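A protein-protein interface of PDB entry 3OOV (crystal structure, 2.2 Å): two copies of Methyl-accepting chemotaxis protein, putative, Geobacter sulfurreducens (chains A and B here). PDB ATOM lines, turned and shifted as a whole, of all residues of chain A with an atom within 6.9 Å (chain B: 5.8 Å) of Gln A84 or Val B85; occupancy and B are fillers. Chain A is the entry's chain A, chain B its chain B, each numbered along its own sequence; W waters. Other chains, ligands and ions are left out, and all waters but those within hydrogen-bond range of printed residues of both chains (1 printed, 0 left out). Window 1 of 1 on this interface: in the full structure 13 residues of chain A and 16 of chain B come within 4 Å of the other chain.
Of the 16 printed residues of chain A, 7 touch a printed residue of chain B.
Hydrophobic or aromatic side chains of chain A that line the printed part of chain B: Tyr A86 and Met A87.
Of the 15 printed residues of chain B, 8 touch a printed residue of chain A.
Hydrophobic or aromatic side chains of chain B within 4 Å of the printed part of chain A: Tyr B86, Ile B88, Tyr B94 and Phe B98.
Water W1 lies within hydrogen-bond range of O of Val B85 (2.7 Å) and O of Val A85 (2.9 Å).
CE1 of Tyr B94 touches O of Asp A82, 3.4 Å away.
Phe B98 touches Asp A82 (CZ to CB, 3.5 Å).
Gln A84 touches Val B85.
OE1 of Gln A84 touches CA of Tyr B86 (3.3 Å).
Gln A84 touches Ile B88.
O of Val A85 touches OE1 of Gln B84 (3.6 Å).
Tyr A86 touches Gln B84.
Tyr B86 touches Tyr A86 (OH to OH, 3.5 Å).
Gln A84 touches just these residues of chain B: Val B85, Tyr B86, Met B87 and Ile B88.
Val B85 touches one residue of chain A.
Of the printed residues of chain A, Lys B150 touches Asp A143.
Printed residues of chain B within 4 Å of Asp A82: Tyr B94 (3.4 Å) and Phe B98 (3.5 Å).
Of the printed residues of chain B, Asp A143 touches Lys B150.
The nearest printed residue of chain A that does not touch Tyr B94 is Gln A84 (4.1 Å).
Gln A84 touches Val B85, and with the chains exchanged Val A85 touches Gln B84.
Gln A84 touches Tyr B86, and with the chains exchanged Tyr A86 touches Gln B84.
Gln A84 touches Met B87, and with the chains exchanged Met A87 touches Gln B84.
Tyr A86 touches its own counterpart, Tyr B86.
9 positions are printed for both chains.
Of the 12 pairs that touch across the chains among the printed residues, 7 have their exchanged pair printed and touching as well.
O of Tyr B86 is in hydrogen-bond range of N of Ile B117 (2.9 Å).
The backbone carbonyl oxygen (O) of Gln B84 is in hydrogen-bond range of the side-chain sulfur (SG) of Cys B79, at 3.2 Å.
The backbone carbonyl oxygen (O) of Asp A82 sits at hydrogen-bond distance from the side-chain amide nitrogen (NE2) of Gln A84 (3.3 Å).
The side-chain carboxylate of Asp A82 is in hydrogen-bond range of the side-chain hydroxyl of Tyr A86, 2.6 Å away.
The backbone carbonyl oxygen (O) of Gln A84 lies within hydrogen-bond range of the side-chain sulfur (SG) of Cys A79, at 3.2 Å.
O of Ile A117 sits at hydrogen-bond distance from N of Tyr A86 (2.9 Å).
The backbone NH (N) of Met A87 is in hydrogen-bond range of the side-chain amide oxygen (OE1) of Gln B84, 2.9 Å away.
The guanidinium group (NH1) of Arg A83 sits at hydrogen-bond distance from the side-chain hydroxyl (OH) of Tyr B94 (3.4 Å).
The side-chain amide oxygen (OE1) of Gln A84 sits at hydrogen-bond distance from the backbone NH (N) of Met B87, at 2.8 Å.
The side-chain carboxylate (OD1) of Asp A143 lies within salt-bridge range of the side-chain amino group (NZ) of Lys B150 (2.7 Å).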
ATOM      1  N   VAL A  75     -13.051   5.414   3.872  1.00  0.00           N
ATOM      2  CA  VAL A  75     -14.479   5.445   3.773  1.00  0.00           C
ATOM      3  C   VAL A  75     -15.040   6.822   4.153  1.00  0.00           C
ATOM      4  O   VAL A  75     -16.167   7.137   3.866  1.00  0.00           O
ATOM      5  CB  VAL A  75     -15.109   4.315   4.657  1.00  0.00           C
ATOM      6  CG1 VAL A  75     -14.773   4.530   6.147  1.00  0.00           C
ATOM      7  CG2 VAL A  75     -16.599   4.289   4.467  1.00  0.00           C
ATOM      8  N   LYS A  78     -15.145   8.410   0.891  1.00  0.00           N
ATOM      9  CA  LYS A  78     -16.257   7.840   0.075  1.00  0.00           C
ATOM     10  C   LYS A  78     -17.567   8.345   0.502  1.00  0.00           C
ATOM     11  O   LYS A  78     -18.431   8.605  -0.368  1.00  0.00           O
ATOM     12  CB  LYS A  78     -16.263   6.323   0.061  1.00  0.00           C
ATOM     13  CG  LYS A  78     -15.175   5.756  -0.812  1.00  0.00           C
ATOM     14  CD  LYS A  78     -14.571   4.486  -0.231  1.00  0.00           C
ATOM     15  CE  LYS A  78     -15.538   3.348  -0.393  1.00  0.00           C
ATOM     16  NZ  LYS A  78     -15.835   3.184  -1.903  1.00  0.00           N
ATOM     17  N   CYS A  79     -17.784   8.442   1.835  1.00  0.00           N
ATOM     18  CA  CYS A  79     -19.017   9.061   2.331  1.00  0.00           C
ATOM     19  C   CYS A  79     -19.229  10.474   1.718  1.00  0.00           C
ATOM     20  O   CYS A  79     -20.359  10.853   1.267  1.00  0.00           O
ATOM     21  CB  CYS A  79     -18.970   9.222   3.873  1.00  0.00           C
ATOM     22  SG  CYS A  79     -20.421  10.043   4.537  1.00  0.00           S
ATOM     23  N   PHE A  80     -18.168  11.276   1.798  1.00  0.00           N
ATOM     24  CA  PHE A  80     -18.230  12.675   1.366  1.00  0.00           C
ATOM     25  C   PHE A  80     -18.544  12.736  -0.169  1.00  0.00           C
ATOM     26  O   PHE A  80     -19.463  13.455  -0.589  1.00  0.00           O
ATOM     27  CB  PHE A  80     -16.895  13.371   1.626  1.00  0.00           C
ATOM     28  CG  PHE A  80     -16.902  14.825   1.260  1.00  0.00           C
ATOM     29  CD1 PHE A  80     -17.346  15.785   2.199  1.00  0.00           C
ATOM     30  CD2 PHE A  80     -16.467  15.241   0.000  1.00  0.00           C
ATOM     31  CE1 PHE A  80     -17.370  17.132   1.865  1.00  0.00           C
ATOM     32  CE2 PHE A  80     -16.470  16.593  -0.348  1.00  0.00           C
ATOM     33  CZ  PHE A  80     -16.900  17.542   0.596  1.00  0.00           C
ATOM     34  N   THR A  81     -17.799  11.961  -0.958  1.00  0.00           N
ATOM     35  CA  THR A  81     -17.958  11.928  -2.428  1.00  0.00           C
ATOM     36  C   THR A  81     -19.353  11.414  -2.886  1.00  0.00           C
ATOM     37  O   THR A  81     -19.991  11.990  -3.759  1.00  0.00           O
ATOM     38  CB  THR A  81     -16.773  11.139  -3.055  1.00  0.00           C
ATOM     39  OG1 THR A  81     -15.539  11.708  -2.556  1.00  0.00           O
ATOM     40  CG2 THR A  81     -16.653  11.390  -4.498  1.00  0.00           C
ATOM     41  N   ASP A  82     -19.848  10.350  -2.264  1.00  0.00           N
ATOM     42  CA  ASP A  82     -21.070   9.674  -2.704  1.00  0.00           C
ATOM     43  C   ASP A  82     -22.305  10.175  -1.969  1.00  0.00           C
ATOM     44  O   ASP A  82     -23.427   9.722  -2.235  1.00  0.00           O
ATOM     45  CB  ASP A  82     -20.976   8.168  -2.405  1.00  0.00           C
ATOM     46  CG  ASP A  82     -19.829   7.457  -3.117  1.00  0.00           C
ATOM     47  OD1 ASP A  82     -19.146   8.053  -3.970  1.00  0.00           O
ATOM     48  OD2 ASP A  82     -19.584   6.252  -2.777  1.00  0.00           O
ATOM     49  N   ARG A  83     -22.108  11.027  -0.957  1.00  0.00           N
ATOM     50  CA  ARG A  83     -23.225  11.508  -0.077  1.00  0.00           C
ATOM     51  C   ARG A  83     -24.037  10.322   0.441  1.00  0.00           C
ATOM     52  O   ARG A  83     -25.253  10.341   0.494  1.00  0.00           O
ATOM     53  CB  ARG A  83     -24.123  12.526  -0.814  1.00  0.00           C
ATOM     54  CG  ARG A  83     -23.388  13.776  -1.267  1.00  0.00           C
ATOM     55  CD  ARG A  83     -24.374  14.793  -1.952  1.00  0.00           C
ATOM     56  NE  ARG A  83     -24.570  14.507  -3.383  1.00  0.00           N
ATOM     57  CZ  ARG A  83     -25.741  14.239  -3.953  1.00  0.00           C
ATOM     58  NH1 ARG A  83     -26.879  14.213  -3.240  1.00  0.00           N
ATOM     59  NH2 ARG A  83     -25.759  13.997  -5.260  1.00  0.00           N
ATOM     60  N   GLN A  84     -23.354   9.265   0.813  1.00  0.00           N
ATOM     61  CA  GLN A  84     -24.031   8.080   1.277  1.00  0.00           C
ATOM     62  C   GLN A  84     -23.599   7.787   2.741  1.00  0.00           C
ATOM     63  O   GLN A  84     -22.431   7.959   3.085  1.00  0.00           O
ATOM     64  CB  GLN A  84     -23.737   6.897   0.339  1.00  0.00           C
ATOM     65  CG  GLN A  84     -24.967   5.976   0.019  1.00  0.00           C
ATOM     66  CD  GLN A  84     -26.150   6.689  -0.663  1.00  0.00           C
ATOM     67  OE1 GLN A  84     -27.320   6.419  -0.340  1.00  0.00           O
ATOM     68  NE2 GLN A  84     -25.852   7.623  -1.613  1.00  0.00           N
ATOM     69  N   VAL A  85     -24.560   7.398   3.580  1.00  0.00           N
ATOM     70  CA  VAL A  85     -24.295   6.812   4.917  1.00  0.00           C
ATOM     71  C   VAL A  85     -23.554   5.512   4.706  1.00  0.00           C
ATOM     72  O   VAL A  85     -24.028   4.632   3.920  1.00  0.00           O
ATOM     73  CB  VAL A  85     -25.584   6.571   5.690  1.00  0.00           C
ATOM     74  CG1 VAL A  85     -25.291   5.894   7.077  1.00  0.00           C
ATOM     75  CG2 VAL A  85     -26.327   7.888   5.886  1.00  0.00           C
ATOM     76  N   TYR A  86     -22.383   5.403   5.338  1.00  0.00           N
ATOM     77  CA  TYR A  86     -21.621   4.145   5.365  1.00  0.00           C
ATOM     78  C   TYR A  86     -21.724   3.577   6.764  1.00  0.00           C
ATOM     79  O   TYR A  86     -21.291   4.209   7.722  1.00  0.00           O
ATOM     80  CB  TYR A  86     -20.139   4.292   4.966  1.00  0.00           C
ATOM     81  CG  TYR A  86     -19.943   4.327   3.455  1.00  0.00           C
ATOM     82  CD1 TYR A  86     -19.672   3.170   2.719  1.00  0.00           C
ATOM     83  CD2 TYR A  86     -20.084   5.542   2.740  1.00  0.00           C
ATOM     84  CE1 TYR A  86     -19.473   3.241   1.292  1.00  0.00           C
ATOM     85  CE2 TYR A  86     -19.966   5.601   1.318  1.00  0.00           C
ATOM     86  CZ  TYR A  86     -19.649   4.465   0.612  1.00  0.00           C
ATOM     87  OH  TYR A  86     -19.550   4.583  -0.783  1.00  0.00           O
ATOM     88  N   MET A  87     -22.348   2.420   6.896  1.00  0.00           N
ATOM     89  CA  MET A  87     -22.429   1.831   8.205  1.00  0.00           C
ATOM     90  C   MET A  87     -21.522   0.634   8.224  1.00  0.00           C
ATOM     91  O   MET A  87     -21.697  -0.292   7.438  1.00  0.00           O
ATOM     92  CB  MET A  87     -23.867   1.601   8.685  1.00  0.00           C
ATOM     93  CG  MET A  87     -24.823   0.925   7.755  1.00  0.00           C
ATOM     94  SD  MET A  87     -26.665   0.943   8.579  1.00  0.00           S
ATOM     95  CE  MET A  87     -26.146   0.543  10.397  1.00  0.00           C
ATOM     96  N   ILE A 117     -20.444   6.609   9.186  1.00  0.00           N
ATOM     97  CA  ILE A 117     -20.120   7.956   8.609  1.00  0.00           C
ATOM     98  C   ILE A 117     -21.350   8.419   7.843  1.00  0.00           C
ATOM     99  O   ILE A 117     -21.914   7.681   7.013  1.00  0.00           O
ATOM    100  CB  ILE A 117     -18.963   7.940   7.607  1.00  0.00           C
ATOM    101  CG1 ILE A 117     -17.844   6.931   7.968  1.00  0.00           C
ATOM    102  CG2 ILE A 117     -18.495   9.407   7.341  1.00  0.00           C
ATOM    103  CD1 ILE A 117     -17.011   7.296   9.335  1.00  0.00           C
ATOM    104  N   CYS A 118     -21.734   9.653   8.109  1.00  0.00           N
ATOM    105  CA  CYS A 118     -22.970  10.206   7.605  1.00  0.00           C
ATOM    106  C   CYS A 118     -22.640  11.597   7.000  1.00  0.00           C
ATOM    107  O   CYS A 118     -21.974  12.382   7.639  1.00  0.00           O
ATOM    108  CB  CYS A 118     -23.985  10.295   8.725  1.00  0.00           C
ATOM    109  SG  CYS A 118     -25.447  11.206   8.207  1.00  0.00           S
ATOM    110  N   PRO A 119     -23.023  11.849   5.748  1.00  0.00           N
ATOM    111  CA  PRO A 119     -22.608  13.104   5.084  1.00  0.00           C
ATOM    112  C   PRO A 119     -23.470  14.238   5.620  1.00  0.00           C
ATOM    113  O   PRO A 119     -24.601  13.990   6.027  1.00  0.00           O
ATOM    114  CB  PRO A 119     -22.944  12.851   3.605  1.00  0.00           C
ATOM    115  CG  PRO A 119     -24.240  11.889   3.677  1.00  0.00           C
ATOM    116  CD  PRO A 119     -23.936  11.023   4.915  1.00  0.00           C
ATOM    117  N   VAL A 121     -25.258  17.366   4.180  1.00  0.00           N
ATOM    118  CA  VAL A 121     -25.522  17.653   2.776  1.00  0.00           C
ATOM    119  C   VAL A 121     -26.292  18.932   2.730  1.00  0.00           C
ATOM    120  O   VAL A 121     -27.318  19.101   3.422  1.00  0.00           O
ATOM    121  CB  VAL A 121     -26.315  16.499   2.045  1.00  0.00           C
ATOM    122  CG1 VAL A 121     -26.675  16.905   0.588  1.00  0.00           C
ATOM    123  CG2 VAL A 121     -25.503  15.170   2.033  1.00  0.00           C
ATOM    124  N   ASP A 143     -29.820   0.600  12.174  1.00  0.00           N
ATOM    125  CA  ASP A 143     -30.626   1.527  11.372  1.00  0.00           C
ATOM    126  C   ASP A 143     -31.253   2.582  12.221  1.00  0.00           C
ATOM    127  O   ASP A 143     -31.374   3.710  11.781  1.00  0.00           O
ATOM    128  CB  ASP A 143     -31.698   0.781  10.570  1.00  0.00           C
ATOM    129  CG  ASP A 143     -31.116  -0.022   9.395  1.00  0.00           C
ATOM    130  OD1 ASP A 143     -29.939   0.163   8.971  1.00  0.00           O
ATOM    131  OD2 ASP A 143     -31.856  -0.868   8.860  1.00  0.00           O
ATOM    132  N   CYS B  79     -22.991  -1.380  -4.776  1.00  0.00           N
ATOM    133  CA  CYS B  79     -23.759  -2.138  -3.755  1.00  0.00           C
ATOM    134  C   CYS B  79     -23.240  -3.551  -3.508  1.00  0.00           C
ATOM    135  O   CYS B  79     -23.045  -3.933  -2.348  1.00  0.00           O
ATOM    136  CB  CYS B  79     -25.213  -2.210  -4.135  1.00  0.00           C
ATOM    137  SG  CYS B  79     -26.369  -2.708  -2.794  1.00  0.00           S
ATOM    138  N   ARG B  83     -21.835  -3.483   0.121  1.00  0.00           N
ATOM    139  CA  ARG B  83     -23.012  -3.843   0.932  1.00  0.00           C
ATOM    140  C   ARG B  83     -23.668  -2.672   1.651  1.00  0.00           C
ATOM    141  O   ARG B  83     -24.216  -2.819   2.734  1.00  0.00           O
ATOM    142  CB  ARG B  83     -22.713  -4.996   1.916  1.00  0.00           C
ATOM    143  CG  ARG B  83     -21.887  -6.065   1.316  1.00  0.00           C
ATOM    144  CD  ARG B  83     -21.641  -7.200   2.327  1.00  0.00           C
ATOM    145  NE  ARG B  83     -20.654  -6.898   3.373  1.00  0.00           N
ATOM    146  CZ  ARG B  83     -19.335  -6.963   3.199  1.00  0.00           C
ATOM    147  NH1 ARG B  83     -18.819  -7.267   1.999  1.00  0.00           N
ATOM    148  NH2 ARG B  83     -18.521  -6.721   4.227  1.00  0.00           N
ATOM    149  N   GLN B  84     -23.688  -1.512   1.029  1.00  0.00           N
ATOM    150  CA  GLN B  84     -24.423  -0.413   1.591  1.00  0.00           C
ATOM    151  C   GLN B  84     -25.760  -0.299   0.880  1.00  0.00           C
ATOM    152  O   GLN B  84     -25.903  -0.756  -0.258  1.00  0.00           O
ATOM    153  CB  GLN B  84     -23.596   0.911   1.439  1.00  0.00           C
ATOM    154  CG  GLN B  84     -22.231   0.934   2.102  1.00  0.00           C
ATOM    155  CD  GLN B  84     -22.279   0.561   3.580  1.00  0.00           C
ATOM    156  OE1 GLN B  84     -22.963   1.193   4.367  1.00  0.00           O
ATOM    157  NE2 GLN B  84     -21.617  -0.506   3.928  1.00  0.00           N
ATOM    158  N   VAL B  85     -26.707   0.361   1.516  1.00  0.00           N
ATOM    159  CA  VAL B  85     -27.928   0.764   0.901  1.00  0.00           C
ATOM    160  C   VAL B  85     -27.727   2.142   0.217  1.00  0.00           C
ATOM    161  O   VAL B  85     -27.253   3.071   0.878  1.00  0.00           O
ATOM    162  CB  VAL B  85     -29.018   0.934   2.025  1.00  0.00           C
ATOM    163  CG1 VAL B  85     -30.302   1.490   1.443  1.00  0.00           C
ATOM    164  CG2 VAL B  85     -29.276  -0.430   2.736  1.00  0.00           C
ATOM    165  N   TYR B  86     -28.049   2.280  -1.080  1.00  0.00           N
ATOM    166  CA  TYR B  86     -28.005   3.578  -1.771  1.00  0.00           C
ATOM    167  C   TYR B  86     -29.385   4.151  -1.989  1.00  0.00           C
ATOM    168  O   TYR B  86     -30.248   3.509  -2.562  1.00  0.00           O
ATOM    169  CB  TYR B  86     -27.247   3.489  -3.101  1.00  0.00           C
ATOM    170  CG  TYR B  86     -25.779   3.144  -2.917  1.00  0.00           C
ATOM    171  CD1 TYR B  86     -24.805   4.133  -2.964  1.00  0.00           C
ATOM    172  CD2 TYR B  86     -25.374   1.857  -2.684  1.00  0.00           C
ATOM    173  CE1 TYR B  86     -23.423   3.813  -2.756  1.00  0.00           C
ATOM    174  CE2 TYR B  86     -24.019   1.530  -2.520  1.00  0.00           C
ATOM    175  CZ  TYR B  86     -23.061   2.547  -2.527  1.00  0.00           C
ATOM    176  OH  TYR B  86     -21.704   2.270  -2.336  1.00  0.00           O
ATOM    177  N   MET B  87     -29.608   5.352  -1.476  1.00  0.00           N
ATOM    178  CA  MET B  87     -30.833   6.095  -1.772  1.00  0.00           C
ATOM    179  C   MET B  87     -30.482   7.224  -2.771  1.00  0.00           C
ATOM    180  O   MET B  87     -29.709   8.125  -2.464  1.00  0.00           O
ATOM    181  CB  MET B  87     -31.440   6.657  -0.498  1.00  0.00           C
ATOM    182  CG  MET B  87     -31.327   5.758   0.760  1.00  0.00           C
ATOM    183  SD  MET B  87     -32.356   6.585   2.236  1.00  0.00           S
ATOM    184  CE  MET B  87     -33.829   7.334   1.091  1.00  0.00           C
ATOM    185  N   ILE B  88     -30.953   7.125  -4.003  1.00  0.00           N
ATOM    186  CA  ILE B  88     -30.510   8.053  -5.061  1.00  0.00           C
ATOM    187  C   ILE B  88     -31.694   8.960  -5.448  1.00  0.00           C
ATOM    188  O   ILE B  88     -32.774   8.459  -5.734  1.00  0.00           O
ATOM    189  CB  ILE B  88     -29.901   7.275  -6.283  1.00  0.00           C
ATOM    190  CG1 ILE B  88     -28.768   6.317  -5.847  1.00  0.00           C
ATOM    191  CG2 ILE B  88     -29.419   8.243  -7.373  1.00  0.00           C
ATOM    192  CD1 ILE B  88     -27.646   6.987  -5.056  1.00  0.00           C
ATOM    193  N   TYR B  94     -24.688  12.733  -9.081  1.00  0.00           N
ATOM    194  CA  TYR B  94     -23.760  11.909  -8.297  1.00  0.00           C
ATOM    195  C   TYR B  94     -22.451  11.659  -9.034  1.00  0.00           C
ATOM    196  O   TYR B  94     -22.352  11.981 -10.147  1.00  0.00           O
ATOM    197  CB  TYR B  94     -24.445  10.600  -7.922  1.00  0.00           C
ATOM    198  CG  TYR B  94     -25.431  10.747  -6.775  1.00  0.00           C
ATOM    199  CD1 TYR B  94     -25.041  10.496  -5.434  1.00  0.00           C
ATOM    200  CD2 TYR B  94     -26.749  11.118  -7.031  1.00  0.00           C
ATOM    201  CE1 TYR B  94     -25.959  10.667  -4.376  1.00  0.00           C
ATOM    202  CE2 TYR B  94     -27.680  11.259  -5.990  1.00  0.00           C
ATOM    203  CZ  TYR B  94     -27.288  11.023  -4.691  1.00  0.00           C
ATOM    204  OH  TYR B  94     -28.259  11.188  -3.738  1.00  0.00           O
ATOM    205  N   PHE B  98     -21.621   6.299 -10.448  1.00  0.00           N
ATOM    206  CA  PHE B  98     -23.011   5.911 -10.158  1.00  0.00           C
ATOM    207  C   PHE B  98     -23.849   5.509 -11.365  1.00  0.00           C
ATOM    208  O   PHE B  98     -24.593   4.547 -11.265  1.00  0.00           O
ATOM    209  CB  PHE B  98     -23.781   6.972  -9.370  1.00  0.00           C
ATOM    210  CG  PHE B  98     -23.493   6.968  -7.838  1.00  0.00           C
ATOM    211  CD1 PHE B  98     -22.168   6.968  -7.346  1.00  0.00           C
ATOM    212  CD2 PHE B  98     -24.550   7.051  -6.913  1.00  0.00           C
ATOM    213  CE1 PHE B  98     -21.928   7.028  -5.956  1.00  0.00           C
ATOM    214  CE2 PHE B  98     -24.318   7.097  -5.530  1.00  0.00           C
ATOM    215  CZ  PHE B  98     -23.007   7.090  -5.054  1.00  0.00           C
ATOM    216  N   VAL B 116     -33.720   3.166  -4.850  1.00  0.00           N
ATOM    217  CA  VAL B 116     -33.071   2.569  -3.681  1.00  0.00           C
ATOM    218  C   VAL B 116     -32.430   1.233  -4.107  1.00  0.00           C
ATOM    219  O   VAL B 116     -33.087   0.406  -4.794  1.00  0.00           O
ATOM    220  CB  VAL B 116     -34.097   2.335  -2.559  1.00  0.00           C
ATOM    221  CG1 VAL B 116     -33.413   1.740  -1.331  1.00  0.00           C
ATOM    222  CG2 VAL B 116     -34.776   3.611  -2.204  1.00  0.00           C
ATOM    223  N   ILE B 117     -31.139   1.051  -3.812  1.00  0.00           N
ATOM    224  CA  ILE B 117     -30.505  -0.246  -4.024  1.00  0.00           C
ATOM    225  C   ILE B 117     -30.239  -0.796  -2.618  1.00  0.00           C
ATOM    226  O   ILE B 117     -29.671  -0.068  -1.744  1.00  0.00           O
ATOM    227  CB  ILE B 117     -29.202  -0.140  -4.764  1.00  0.00           C
ATOM    228  CG1 ILE B 117     -29.248   0.817  -5.995  1.00  0.00           C
ATOM    229  CG2 ILE B 117     -28.738  -1.499  -5.187  1.00  0.00           C
ATOM    230  CD1 ILE B 117     -30.207   0.339  -7.179  1.00  0.00           C
ATOM    231  N   CYS B 118     -30.647  -2.042  -2.381  1.00  0.00           N
ATOM    232  CA  CYS B 118     -30.492  -2.681  -1.065  1.00  0.00           C
ATOM    233  C   CYS B 118     -29.866  -4.045  -1.304  1.00  0.00           C
ATOM    234  O   CYS B 118     -30.411  -4.804  -2.092  1.00  0.00           O
ATOM    235  CB  CYS B 118     -31.868  -2.822  -0.373  1.00  0.00           C
ATOM    236  SG  CYS B 118     -31.705  -3.563   1.232  1.00  0.00           S
ATOM    237  N   PRO B 119     -28.689  -4.340  -0.679  1.00  0.00           N
ATOM    238  CA  PRO B 119     -28.046  -5.636  -0.966  1.00  0.00           C
ATOM    239  C   PRO B 119     -28.793  -6.803  -0.259  1.00  0.00           C
ATOM    240  O   PRO B 119     -29.497  -6.562   0.745  1.00  0.00           O
ATOM    241  CB  PRO B 119     -26.687  -5.508  -0.298  1.00  0.00           C
ATOM    242  CG  PRO B 119     -26.928  -4.611   0.847  1.00  0.00           C
ATOM    243  CD  PRO B 119     -28.006  -3.622   0.409  1.00  0.00           C
ATOM    244  N   VAL B 146     -36.623   2.537   3.149  1.00  0.00           N
ATOM    245  CA  VAL B 146     -35.437   1.719   3.090  1.00  0.00           C
ATOM    246  C   VAL B 146     -35.572   0.475   4.028  1.00  0.00           C
ATOM    247  O   VAL B 146     -35.292  -0.665   3.628  1.00  0.00           O
ATOM    248  CB  VAL B 146     -34.167   2.538   3.471  1.00  0.00           C
ATOM    249  CG1 VAL B 146     -32.941   1.606   3.572  1.00  0.00           C
ATOM    250  CG2 VAL B 146     -33.920   3.651   2.465  1.00  0.00           C
ATOM    251  N   LYS B 150     -35.400  -3.393   3.394  1.00  0.00           N
ATOM    252  CA  LYS B 150     -34.357  -4.214   4.080  1.00  0.00           C
ATOM    253  C   LYS B 150     -34.960  -5.434   4.754  1.00  0.00           C
ATOM    254  O   LYS B 150     -34.424  -6.521   4.652  1.00  0.00           O
ATOM    255  CB  LYS B 150     -33.634  -3.446   5.180  1.00  0.00           C
ATOM    256  CG  LYS B 150     -32.584  -2.544   4.704  1.00  0.00           C
ATOM    257  CD  LYS B 150     -31.467  -2.445   5.778  1.00  0.00           C
ATOM    258  CE  LYS B 150     -30.907  -1.034   5.773  1.00  0.00           C
ATOM    259  NZ  LYS B 150     -29.593  -0.826   6.499  1.00  0.00           N
HETATM  260  O   HOH W   1     -26.758   3.820   3.423  1.00  0.00           O
